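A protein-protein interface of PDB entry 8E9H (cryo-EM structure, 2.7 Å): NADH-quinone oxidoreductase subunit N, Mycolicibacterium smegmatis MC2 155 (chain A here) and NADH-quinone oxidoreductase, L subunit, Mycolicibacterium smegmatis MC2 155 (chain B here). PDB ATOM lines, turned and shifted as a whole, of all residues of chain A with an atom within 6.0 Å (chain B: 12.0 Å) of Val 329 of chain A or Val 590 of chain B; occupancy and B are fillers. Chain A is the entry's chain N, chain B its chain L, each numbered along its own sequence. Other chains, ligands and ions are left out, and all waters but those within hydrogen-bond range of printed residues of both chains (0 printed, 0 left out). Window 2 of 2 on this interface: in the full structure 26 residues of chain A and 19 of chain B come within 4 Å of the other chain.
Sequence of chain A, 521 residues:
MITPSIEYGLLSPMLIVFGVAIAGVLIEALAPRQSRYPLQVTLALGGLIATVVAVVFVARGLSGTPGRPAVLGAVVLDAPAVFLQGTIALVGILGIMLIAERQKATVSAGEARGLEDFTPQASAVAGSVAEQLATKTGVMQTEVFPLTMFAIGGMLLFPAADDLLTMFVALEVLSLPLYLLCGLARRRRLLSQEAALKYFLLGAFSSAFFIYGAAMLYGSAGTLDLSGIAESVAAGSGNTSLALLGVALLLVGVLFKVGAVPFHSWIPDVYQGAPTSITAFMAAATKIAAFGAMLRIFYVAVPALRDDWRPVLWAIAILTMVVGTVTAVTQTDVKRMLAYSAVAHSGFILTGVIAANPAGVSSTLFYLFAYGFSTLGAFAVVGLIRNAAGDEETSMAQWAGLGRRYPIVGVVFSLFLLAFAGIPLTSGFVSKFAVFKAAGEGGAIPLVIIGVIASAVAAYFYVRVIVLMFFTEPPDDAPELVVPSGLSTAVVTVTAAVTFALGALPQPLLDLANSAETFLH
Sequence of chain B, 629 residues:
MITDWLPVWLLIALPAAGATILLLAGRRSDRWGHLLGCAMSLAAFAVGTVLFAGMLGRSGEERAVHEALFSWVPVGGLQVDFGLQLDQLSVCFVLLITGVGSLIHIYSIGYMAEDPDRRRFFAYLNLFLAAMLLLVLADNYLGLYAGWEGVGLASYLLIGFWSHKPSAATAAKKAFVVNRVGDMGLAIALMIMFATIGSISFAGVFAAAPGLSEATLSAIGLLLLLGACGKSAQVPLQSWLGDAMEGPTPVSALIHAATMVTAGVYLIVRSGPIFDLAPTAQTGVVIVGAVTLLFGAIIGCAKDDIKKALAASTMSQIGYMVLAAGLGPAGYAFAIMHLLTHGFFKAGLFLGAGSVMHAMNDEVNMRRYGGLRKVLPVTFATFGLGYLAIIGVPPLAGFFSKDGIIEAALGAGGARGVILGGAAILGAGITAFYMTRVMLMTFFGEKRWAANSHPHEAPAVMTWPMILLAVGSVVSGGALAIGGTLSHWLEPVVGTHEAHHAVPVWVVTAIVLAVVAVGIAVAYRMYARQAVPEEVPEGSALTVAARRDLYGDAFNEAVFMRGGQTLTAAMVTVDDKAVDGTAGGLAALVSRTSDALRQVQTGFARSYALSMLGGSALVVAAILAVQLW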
ATOM      1  N   GLY A 324       0.006 -28.973  19.119  1.00  0.00           N
ATOM      2  CA  GLY A 324      -0.179 -27.533  19.078  1.00  0.00           C
ATOM      3  C   GLY A 324      -1.187 -27.057  20.105  1.00  0.00           C
ATOM      4  O   GLY A 324      -1.021 -26.000  20.714  1.00  0.00           O
ATOM      5  N   THR A 325      -2.249 -27.836  20.311  1.00  0.00           N
ATOM      6  CA  THR A 325      -3.301 -27.411  21.228  1.00  0.00           C
ATOM      7  C   THR A 325      -2.967 -27.798  22.661  1.00  0.00           C
ATOM      8  O   THR A 325      -3.036 -26.964  23.571  1.00  0.00           O
ATOM      9  CB  THR A 325      -4.636 -28.019  20.808  1.00  0.00           C
ATOM     10  OG1 THR A 325      -4.505 -29.440  20.704  1.00  0.00           O
ATOM     11  CG2 THR A 325      -5.076 -27.455  19.473  1.00  0.00           C
ATOM     12  N   VAL A 326      -2.587 -29.056  22.880  1.00  0.00           N
ATOM     13  CA  VAL A 326      -2.344 -29.524  24.239  1.00  0.00           C
ATOM     14  C   VAL A 326      -1.262 -28.688  24.901  1.00  0.00           C
ATOM     15  O   VAL A 326      -1.348 -28.364  26.091  1.00  0.00           O
ATOM     16  CB  VAL A 326      -1.981 -31.018  24.233  1.00  0.00           C
ATOM     17  CG1 VAL A 326      -1.635 -31.481  25.630  1.00  0.00           C
ATOM     18  CG2 VAL A 326      -3.130 -31.834  23.676  1.00  0.00           C
ATOM     19  N   THR A 327      -0.228 -28.321  24.147  1.00  0.00           N
ATOM     20  CA  THR A 327       0.820 -27.485  24.717  1.00  0.00           C
ATOM     21  C   THR A 327       0.282 -26.130  25.146  1.00  0.00           C
ATOM     22  O   THR A 327       0.680 -25.610  26.194  1.00  0.00           O
ATOM     23  CB  THR A 327       1.953 -27.300  23.714  1.00  0.00           C
ATOM     24  OG1 THR A 327       2.290 -28.563  23.131  1.00  0.00           O
ATOM     25  CG2 THR A 327       3.174 -26.721  24.400  1.00  0.00           C
ATOM     26  N   ALA A 328      -0.619 -25.543  24.358  1.00  0.00           N
ATOM     27  CA  ALA A 328      -1.169 -24.239  24.705  1.00  0.00           C
ATOM     28  C   ALA A 328      -1.991 -24.276  25.981  1.00  0.00           C
ATOM     29  O   ALA A 328      -2.201 -23.228  26.597  1.00  0.00           O
ATOM     30  CB  ALA A 328      -2.034 -23.713  23.564  1.00  0.00           C
ATOM     31  N   VAL A 329      -2.459 -25.455  26.392  1.00  0.00           N
ATOM     32  CA  VAL A 329      -3.370 -25.538  27.530  1.00  0.00           C
ATOM     33  C   VAL A 329      -2.721 -24.945  28.772  1.00  0.00           C
ATOM     34  O   VAL A 329      -3.328 -24.146  29.493  1.00  0.00           O
ATOM     35  CB  VAL A 329      -3.800 -26.995  27.762  1.00  0.00           C
ATOM     36  CG1 VAL A 329      -4.441 -27.148  29.126  1.00  0.00           C
ATOM     37  CG2 VAL A 329      -4.755 -27.436  26.674  1.00  0.00           C
ATOM     38  N   THR A 330      -1.472 -25.321  29.035  1.00  0.00           N
ATOM     39  CA  THR A 330      -0.813 -24.907  30.265  1.00  0.00           C
ATOM     40  C   THR A 330      -0.065 -23.589  30.130  1.00  0.00           C
ATOM     41  O   THR A 330       0.493 -23.109  31.121  1.00  0.00           O
ATOM     42  CB  THR A 330       0.158 -25.993  30.722  1.00  0.00           C
ATOM     43  OG1 THR A 330       0.561 -25.742  32.074  1.00  0.00           O
ATOM     44  CG2 THR A 330       1.383 -26.024  29.829  1.00  0.00           C
ATOM     45  N   GLN A 331      -0.037 -22.993  28.940  1.00  0.00           N
ATOM     46  CA  GLN A 331       0.720 -21.767  28.730  1.00  0.00           C
ATOM     47  C   GLN A 331       0.190 -20.640  29.604  1.00  0.00           C
ATOM     48  O   GLN A 331      -1.017 -20.543  29.839  1.00  0.00           O
ATOM     49  CB  GLN A 331       0.670 -21.355  27.261  1.00  0.00           C
ATOM     50  CG  GLN A 331       1.481 -22.251  26.344  1.00  0.00           C
ATOM     51  CD  GLN A 331       2.964 -22.261  26.665  1.00  0.00           C
ATOM     52  OE1 GLN A 331       3.478 -21.319  27.267  1.00  0.00           O
ATOM     53  NE2 GLN A 331       3.661 -23.325  26.275  1.00  0.00           N
ATOM     54  N   VAL A 457     -10.293 -29.202  22.943  1.00  0.00           N
ATOM     55  CA  VAL A 457      -9.215 -28.956  23.898  1.00  0.00           C
ATOM     56  C   VAL A 457      -8.782 -27.497  23.847  1.00  0.00           C
ATOM     57  O   VAL A 457      -8.585 -26.855  24.885  1.00  0.00           O
ATOM     58  CB  VAL A 457      -8.034 -29.903  23.626  1.00  0.00           C
ATOM     59  CG1 VAL A 457      -6.795 -29.426  24.358  1.00  0.00           C
ATOM     60  CG2 VAL A 457      -8.385 -31.316  24.043  1.00  0.00           C
ATOM     61  N   ALA A 458      -8.625 -26.951  22.641  1.00  0.00           N
ATOM     62  CA  ALA A 458      -8.090 -25.603  22.499  1.00  0.00           C
ATOM     63  C   ALA A 458      -9.073 -24.558  23.003  1.00  0.00           C
ATOM     64  O   ALA A 458      -8.673 -23.457  23.408  1.00  0.00           O
ATOM     65  CB  ALA A 458      -7.734 -25.336  21.039  1.00  0.00           C
ATOM     66  N   TYR A 460     -10.497 -24.558  25.687  1.00  0.00           N
ATOM     67  CA  TYR A 460     -10.198 -24.284  27.087  1.00  0.00           C
ATOM     68  C   TYR A 460      -9.249 -23.105  27.223  1.00  0.00           C
ATOM     69  O   TYR A 460      -9.503 -22.177  27.997  1.00  0.00           O
ATOM     70  CB  TYR A 460      -9.590 -25.508  27.765  1.00  0.00           C
ATOM     71  CG  TYR A 460      -8.922 -25.156  29.075  1.00  0.00           C
ATOM     72  CD1 TYR A 460      -9.647 -25.112  30.254  1.00  0.00           C
ATOM     73  CD2 TYR A 460      -7.573 -24.844  29.129  1.00  0.00           C
ATOM     74  CE1 TYR A 460      -9.050 -24.783  31.447  1.00  0.00           C
ATOM     75  CE2 TYR A 460      -6.967 -24.510  30.319  1.00  0.00           C
ATOM     76  CZ  TYR A 460      -7.710 -24.483  31.475  1.00  0.00           C
ATOM     77  OH  TYR A 460      -7.110 -24.153  32.666  1.00  0.00           O
ATOM     78  N   PHE A 461      -8.128 -23.140  26.507  1.00  0.00           N
ATOM     79  CA  PHE A 461      -7.147 -22.082  26.684  1.00  0.00           C
ATOM     80  C   PHE A 461      -7.540 -20.820  25.935  1.00  0.00           C
ATOM     81  O   PHE A 461      -7.028 -19.741  26.248  1.00  0.00           O
ATOM     82  CB  PHE A 461      -5.758 -22.570  26.267  1.00  0.00           C
ATOM     83  CG  PHE A 461      -5.523 -22.590  24.787  1.00  0.00           C
ATOM     84  CD1 PHE A 461      -5.200 -21.435  24.105  1.00  0.00           C
ATOM     85  CD2 PHE A 461      -5.582 -23.774  24.085  1.00  0.00           C
ATOM     86  CE1 PHE A 461      -4.972 -21.457  22.751  1.00  0.00           C
ATOM     87  CE2 PHE A 461      -5.352 -23.799  22.730  1.00  0.00           C
ATOM     88  CZ  PHE A 461      -5.046 -22.641  22.064  1.00  0.00           C
ATOM     89  N   GLY B 581     -15.594 -37.353  38.446  1.00  0.00           N
ATOM     90  CA  GLY B 581     -14.250 -37.895  38.429  1.00  0.00           C
ATOM     91  C   GLY B 581     -13.715 -38.129  37.034  1.00  0.00           C
ATOM     92  O   GLY B 581     -12.531 -37.921  36.784  1.00  0.00           O
ATOM     93  N   THR B 582     -14.564 -38.584  36.111  1.00  0.00           N
ATOM     94  CA  THR B 582     -14.092 -38.811  34.750  1.00  0.00           C
ATOM     95  C   THR B 582     -13.642 -37.510  34.100  1.00  0.00           C
ATOM     96  O   THR B 582     -12.577 -37.456  33.475  1.00  0.00           O
ATOM     97  CB  THR B 582     -15.184 -39.470  33.910  1.00  0.00           C
ATOM     98  OG1 THR B 582     -16.336 -38.621  33.869  1.00  0.00           O
ATOM     99  CG2 THR B 582     -15.567 -40.816  34.497  1.00  0.00           C
ATOM    100  N   ALA B 583     -14.439 -36.450  34.236  1.00  0.00           N
ATOM    101  CA  ALA B 583     -14.046 -35.164  33.676  1.00  0.00           C
ATOM    102  C   ALA B 583     -12.798 -34.627  34.361  1.00  0.00           C
ATOM    103  O   ALA B 583     -11.907 -34.082  33.701  1.00  0.00           O
ATOM    104  CB  ALA B 583     -15.193 -34.167  33.799  1.00  0.00           C
ATOM    105  N   GLY B 584     -12.717 -34.765  35.684  1.00  0.00           N
ATOM    106  CA  GLY B 584     -11.520 -34.329  36.381  1.00  0.00           C
ATOM    107  C   GLY B 584     -10.286 -35.078  35.923  1.00  0.00           C
ATOM    108  O   GLY B 584      -9.220 -34.489  35.748  1.00  0.00           O
ATOM    109  N   GLY B 585     -10.418 -36.387  35.716  1.00  0.00           N
ATOM    110  CA  GLY B 585      -9.294 -37.169  35.239  1.00  0.00           C
ATOM    111  C   GLY B 585      -8.888 -36.792  33.830  1.00  0.00           C
ATOM    112  O   GLY B 585      -7.700 -36.731  33.516  1.00  0.00           O
ATOM    113  N   LEU B 586      -9.866 -36.541  32.961  1.00  0.00           N
ATOM    114  CA  LEU B 586      -9.540 -36.098  31.609  1.00  0.00           C
ATOM    115  C   LEU B 586      -8.803 -34.768  31.643  1.00  0.00           C
ATOM    116  O   LEU B 586      -7.798 -34.580  30.946  1.00  0.00           O
ATOM    117  CB  LEU B 586     -10.814 -35.987  30.775  1.00  0.00           C
ATOM    118  CG  LEU B 586     -10.605 -35.588  29.315  1.00  0.00           C
ATOM    119  CD1 LEU B 586     -11.589 -36.318  28.421  1.00  0.00           C
ATOM    120  CD2 LEU B 586     -10.744 -34.087  29.138  1.00  0.00           C
ATOM    121  N   ALA B 587      -9.287 -33.826  32.453  1.00  0.00           N
ATOM    122  CA  ALA B 587      -8.621 -32.534  32.553  1.00  0.00           C
ATOM    123  C   ALA B 587      -7.215 -32.686  33.115  1.00  0.00           C
ATOM    124  O   ALA B 587      -6.275 -32.039  32.641  1.00  0.00           O
ATOM    125  CB  ALA B 587      -9.444 -31.586  33.422  1.00  0.00           C
ATOM    126  N   ALA B 588      -7.052 -33.535  34.128  1.00  0.00           N
ATOM    127  CA  ALA B 588      -5.733 -33.748  34.709  1.00  0.00           C
ATOM    128  C   ALA B 588      -4.793 -34.380  33.695  1.00  0.00           C
ATOM    129  O   ALA B 588      -3.611 -34.034  33.627  1.00  0.00           O
ATOM    130  CB  ALA B 588      -5.846 -34.622  35.957  1.00  0.00           C
ATOM    131  N   LEU B 589      -5.300 -35.327  32.906  1.00  0.00           N
ATOM    132  CA  LEU B 589      -4.480 -35.945  31.872  1.00  0.00           C
ATOM    133  C   LEU B 589      -4.047 -34.914  30.843  1.00  0.00           C
ATOM    134  O   LEU B 589      -2.885 -34.888  30.422  1.00  0.00           O
ATOM    135  CB  LEU B 589      -5.255 -37.081  31.208  1.00  0.00           C
ATOM    136  CG  LEU B 589      -4.598 -37.719  29.985  1.00  0.00           C
ATOM    137  CD1 LEU B 589      -3.248 -38.305  30.350  1.00  0.00           C
ATOM    138  CD2 LEU B 589      -5.503 -38.786  29.398  1.00  0.00           C
ATOM    139  N   VAL B 590      -4.971 -34.049  30.427  1.00  0.00           N
ATOM    140  CA  VAL B 590      -4.619 -33.019  29.458  1.00  0.00           C
ATOM    141  C   VAL B 590      -3.574 -32.081  30.042  1.00  0.00           C
ATOM    142  O   VAL B 590      -2.627 -31.688  29.358  1.00  0.00           O
ATOM    143  CB  VAL B 590      -5.872 -32.256  29.000  1.00  0.00           C
ATOM    144  CG1 VAL B 590      -5.477 -31.047  28.180  1.00  0.00           C
ATOM    145  CG2 VAL B 590      -6.769 -33.165  28.189  1.00  0.00           C
ATOM    146  N   SER B 591      -3.726 -31.703  31.312  1.00  0.00           N
ATOM    147  CA  SER B 591      -2.761 -30.801  31.933  1.00  0.00           C
ATOM    148  C   SER B 591      -1.390 -31.456  32.059  1.00  0.00           C
ATOM    149  O   SER B 591      -0.361 -30.819  31.809  1.00  0.00           O
ATOM    150  CB  SER B 591      -3.268 -30.352  33.301  1.00  0.00           C
ATOM    151  OG  SER B 591      -4.515 -29.693  33.187  1.00  0.00           O
ATOM    152  N   ARG B 592      -1.353 -32.726  32.462  1.00  0.00           N
ATOM    153  CA  ARG B 592      -0.078 -33.425  32.578  1.00  0.00           C
ATOM    154  C   ARG B 592       0.596 -33.544  31.220  1.00  0.00           C
ATOM    155  O   ARG B 592       1.807 -33.329  31.090  1.00  0.00           O
ATOM    156  CB  ARG B 592      -0.294 -34.805  33.197  1.00  0.00           C
ATOM    157  N   THR B 593      -0.177 -33.881  30.188  1.00  0.00           N
ATOM    158  CA  THR B 593       0.383 -33.963  28.846  1.00  0.00           C
ATOM    159  C   THR B 593       0.868 -32.600  28.375  1.00  0.00           C
ATOM    160  O   THR B 593       1.898 -32.501  27.704  1.00  0.00           O
ATOM    161  CB  THR B 593      -0.658 -34.521  27.880  1.00  0.00           C
ATOM    162  OG1 THR B 593      -1.189 -35.742  28.403  1.00  0.00           O
ATOM    163  CG2 THR B 593      -0.034 -34.786  26.522  1.00  0.00           C
ATOM    164  N   SER B 594       0.132 -31.540  28.706  1.00  0.00           N
ATOM    165  CA  SER B 594       0.551 -30.199  28.327  1.00  0.00           C
ATOM    166  C   SER B 594       1.873 -29.843  28.985  1.00  0.00           C
ATOM    167  O   SER B 594       2.768 -29.286  28.343  1.00  0.00           O
ATOM    168  CB  SER B 594      -0.528 -29.191  28.712  1.00  0.00           C
ATOM    169  OG  SER B 594      -0.238 -27.912  28.183  1.00  0.00           O
ATOM    170  N   ASP B 595       2.013 -30.154  30.271  1.00  0.00           N
ATOM    171  CA  ASP B 595       3.272 -29.884  30.953  1.00  0.00           C
ATOM    172  C   ASP B 595       4.408 -30.687  30.334  1.00  0.00           C
ATOM    173  O   ASP B 595       5.504 -30.156  30.107  1.00  0.00           O
ATOM    174  CB  ASP B 595       3.136 -30.199  32.440  1.00  0.00           C
ATOM    175  N   ALA B 596       4.164 -31.964  30.037  1.00  0.00           N
ATOM    176  CA  ALA B 596       5.203 -32.787  29.431  1.00  0.00           C
ATOM    177  C   ALA B 596       5.630 -32.222  28.084  1.00  0.00           C
ATOM    178  O   ALA B 596       6.826 -32.097  27.800  1.00  0.00           O
ATOM    179  CB  ALA B 596       4.709 -34.224  29.281  1.00  0.00           C
ATOM    180  N   LEU B 597       4.661 -31.867  27.239  1.00  0.00           N
ATOM    181  CA  LEU B 597       4.990 -31.317  25.929  1.00  0.00           C
ATOM    182  C   LEU B 597       5.719 -29.990  26.056  1.00  0.00           C
ATOM    183  O   LEU B 597       6.683 -29.732  25.329  1.00  0.00           O
ATOM    184  CB  LEU B 597       3.720 -31.145  25.099  1.00  0.00           C
ATOM    185  CG  LEU B 597       3.037 -32.429  24.638  1.00  0.00           C
ATOM    186  CD1 LEU B 597       1.685 -32.110  24.037  1.00  0.00           C
ATOM    187  CD2 LEU B 597       3.901 -33.167  23.636  1.00  0.00           C
ATOM    188  N   ARG B 598       5.276 -29.132  26.974  1.00  0.00           N
ATOM    189  CA  ARG B 598       5.950 -27.857  27.169  1.00  0.00           C
ATOM    190  C   ARG B 598       7.382 -28.062  27.627  1.00  0.00           C
ATOM    191  O   ARG B 598       8.258 -27.250  27.310  1.00  0.00           O
ATOM    192  CB  ARG B 598       5.179 -27.014  28.179  1.00  0.00           C
ATOM    193  CG  ARG B 598       5.717 -25.615  28.342  1.00  0.00           C
ATOM    194  CD  ARG B 598       4.735 -24.743  29.087  1.00  0.00           C
ATOM    195  NE  ARG B 598       4.453 -25.273  30.414  1.00  0.00           N
ATOM    196  CZ  ARG B 598       4.172 -24.533  31.477  1.00  0.00           C
ATOM    197  NH1 ARG B 598       4.123 -23.211  31.410  1.00  0.00           N
ATOM    198  NH2 ARG B 598       3.930 -25.133  32.639  1.00  0.00           N
ATOM    199  N   GLN B 599       7.644 -29.138  28.367  1.00  0.00           N
ATOM    200  CA  GLN B 599       9.021 -29.469  28.708  1.00  0.00           C
ATOM    201  C   GLN B 599       9.869 -29.726  27.469  1.00  0.00           C
ATOM    202  O   GLN B 599      11.094 -29.588  27.533  1.00  0.00           O
ATOM    203  CB  GLN B 599       9.058 -30.689  29.626  1.00  0.00           C
ATOM    204  N   GLN B 601       9.815 -27.868  24.852  1.00  0.00           N
ATOM    205  CA  GLN B 601      10.240 -26.540  24.417  1.00  0.00           C
ATOM    206  C   GLN B 601      11.403 -26.055  25.284  1.00  0.00           C
ATOM    207  O   GLN B 601      11.305 -25.091  26.042  1.00  0.00           O
ATOM    208  CB  GLN B 601       9.064 -25.576  24.475  1.00  0.00           C
ATOM    209  CG  GLN B 601       9.296 -24.266  23.756  1.00  0.00           C
ATOM    210  CD  GLN B 601       9.234 -24.409  22.255  1.00  0.00           C
ATOM    211  OE1 GLN B 601       8.876 -25.465  21.735  1.00  0.00           O
ATOM    212  NE2 GLN B 601       9.582 -23.343  21.547  1.00  0.00           N
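O of Leu 589 of chain B sits at hydrogen-bond distance from OG1 of Thr 593 of chain B (2.8 Å).
Of the printed residues of chain A, Val 590 of chain B touches Val 326 and Val 329. No residue of chain B comes within 4 Å of Thr 325 of chain A. Val 326 of chain A touches just these residues of chain B: Val 590 (3.9 Å), Thr 593 (3.8 Å), Ser 594 (2.4 Å) and Leu 597 (3.7 Å). Gln 331 of chain A touches just one residue of chain B: Arg 598. No residue of chain B comes within 4 Å of Val 457 of chain A. No residue of chain B comes within 4 Å of Ala 458 of chain A. No residue of chain B comes within 4 Å of Tyr 460 of chain A. No residue of chain B comes within 4 Å of Phe 461 of chain A. Of the printed residues of chain A, Arg 598 of chain B touches Thr 330 (3.2 Å) and Gln 331 (3.3 Å). Of the printed residues of chain A, Thr 593 of chain B touches Val 326. Of the printed residues of chain A, Leu 597 of chain B touches Val 326 and Thr 327. Ala 587 of chain B touches none of the printed residues of chain A. The nearest residue of chain B that does not touch Val 329 of chain A is Ser 591 of chain B (4.8 Å). The nearest residue of chain A that does not touch Val 590 of chain B is Val 457 of chain A (4.4 Å). The nearest printed residue of chain A that does not touch Leu 597 of chain B is Gly 324 of chain A (6.1 Å).
The side-chain hydroxyl (OG) of Ser 594 of chain B lies within hydrogen-bond range of the backbone carbonyl oxygen (O) of Val 326 of chain A (2.4 Å). The side-chain hydroxyl of Ser 594 of chain B sits at hydrogen-bond distance from the backbone carbonyl oxygen of Thr 327 of chain A, at 3.2 Å. OG of Ser 594 of chain B lies close to N of Thr 330 of chain A, at 3.0 Å. NH2 of Arg 598 of chain B is in hydrogen-bond range of OG1 of Thr 330 of chain A, 3.5 Å away.
O of Val 590 of chain B touches CG1 of Val 326 of chain A, at 3.9 Å. CG2 of Thr 593 of chain B touches CG1 of Val 326 of chain A, at 3.8 Å. Val 326 of chain A touches Leu 597 of chain B. Leu 597 of chain B touches Thr 327 of chain A. Val 329 of chain A touches Val 590 of chain B. Val 329 of chain A touches Ser 594 of chain B. Gln 331 of chain A touches Arg 598 of chain B (NE2 to CD, 3.3 Å).
Of the 12 printed residues of chain A, 5 touch a printed residue of chain B. Hydrophobic or aromatic side chains of chain B that line the printed part of chain A: Val 590 and Leu 597. Among the printed residues, no Asp or Glu carboxylate lies within 4 Å of a Lys or Arg side-chain nitrogen of the other chain.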
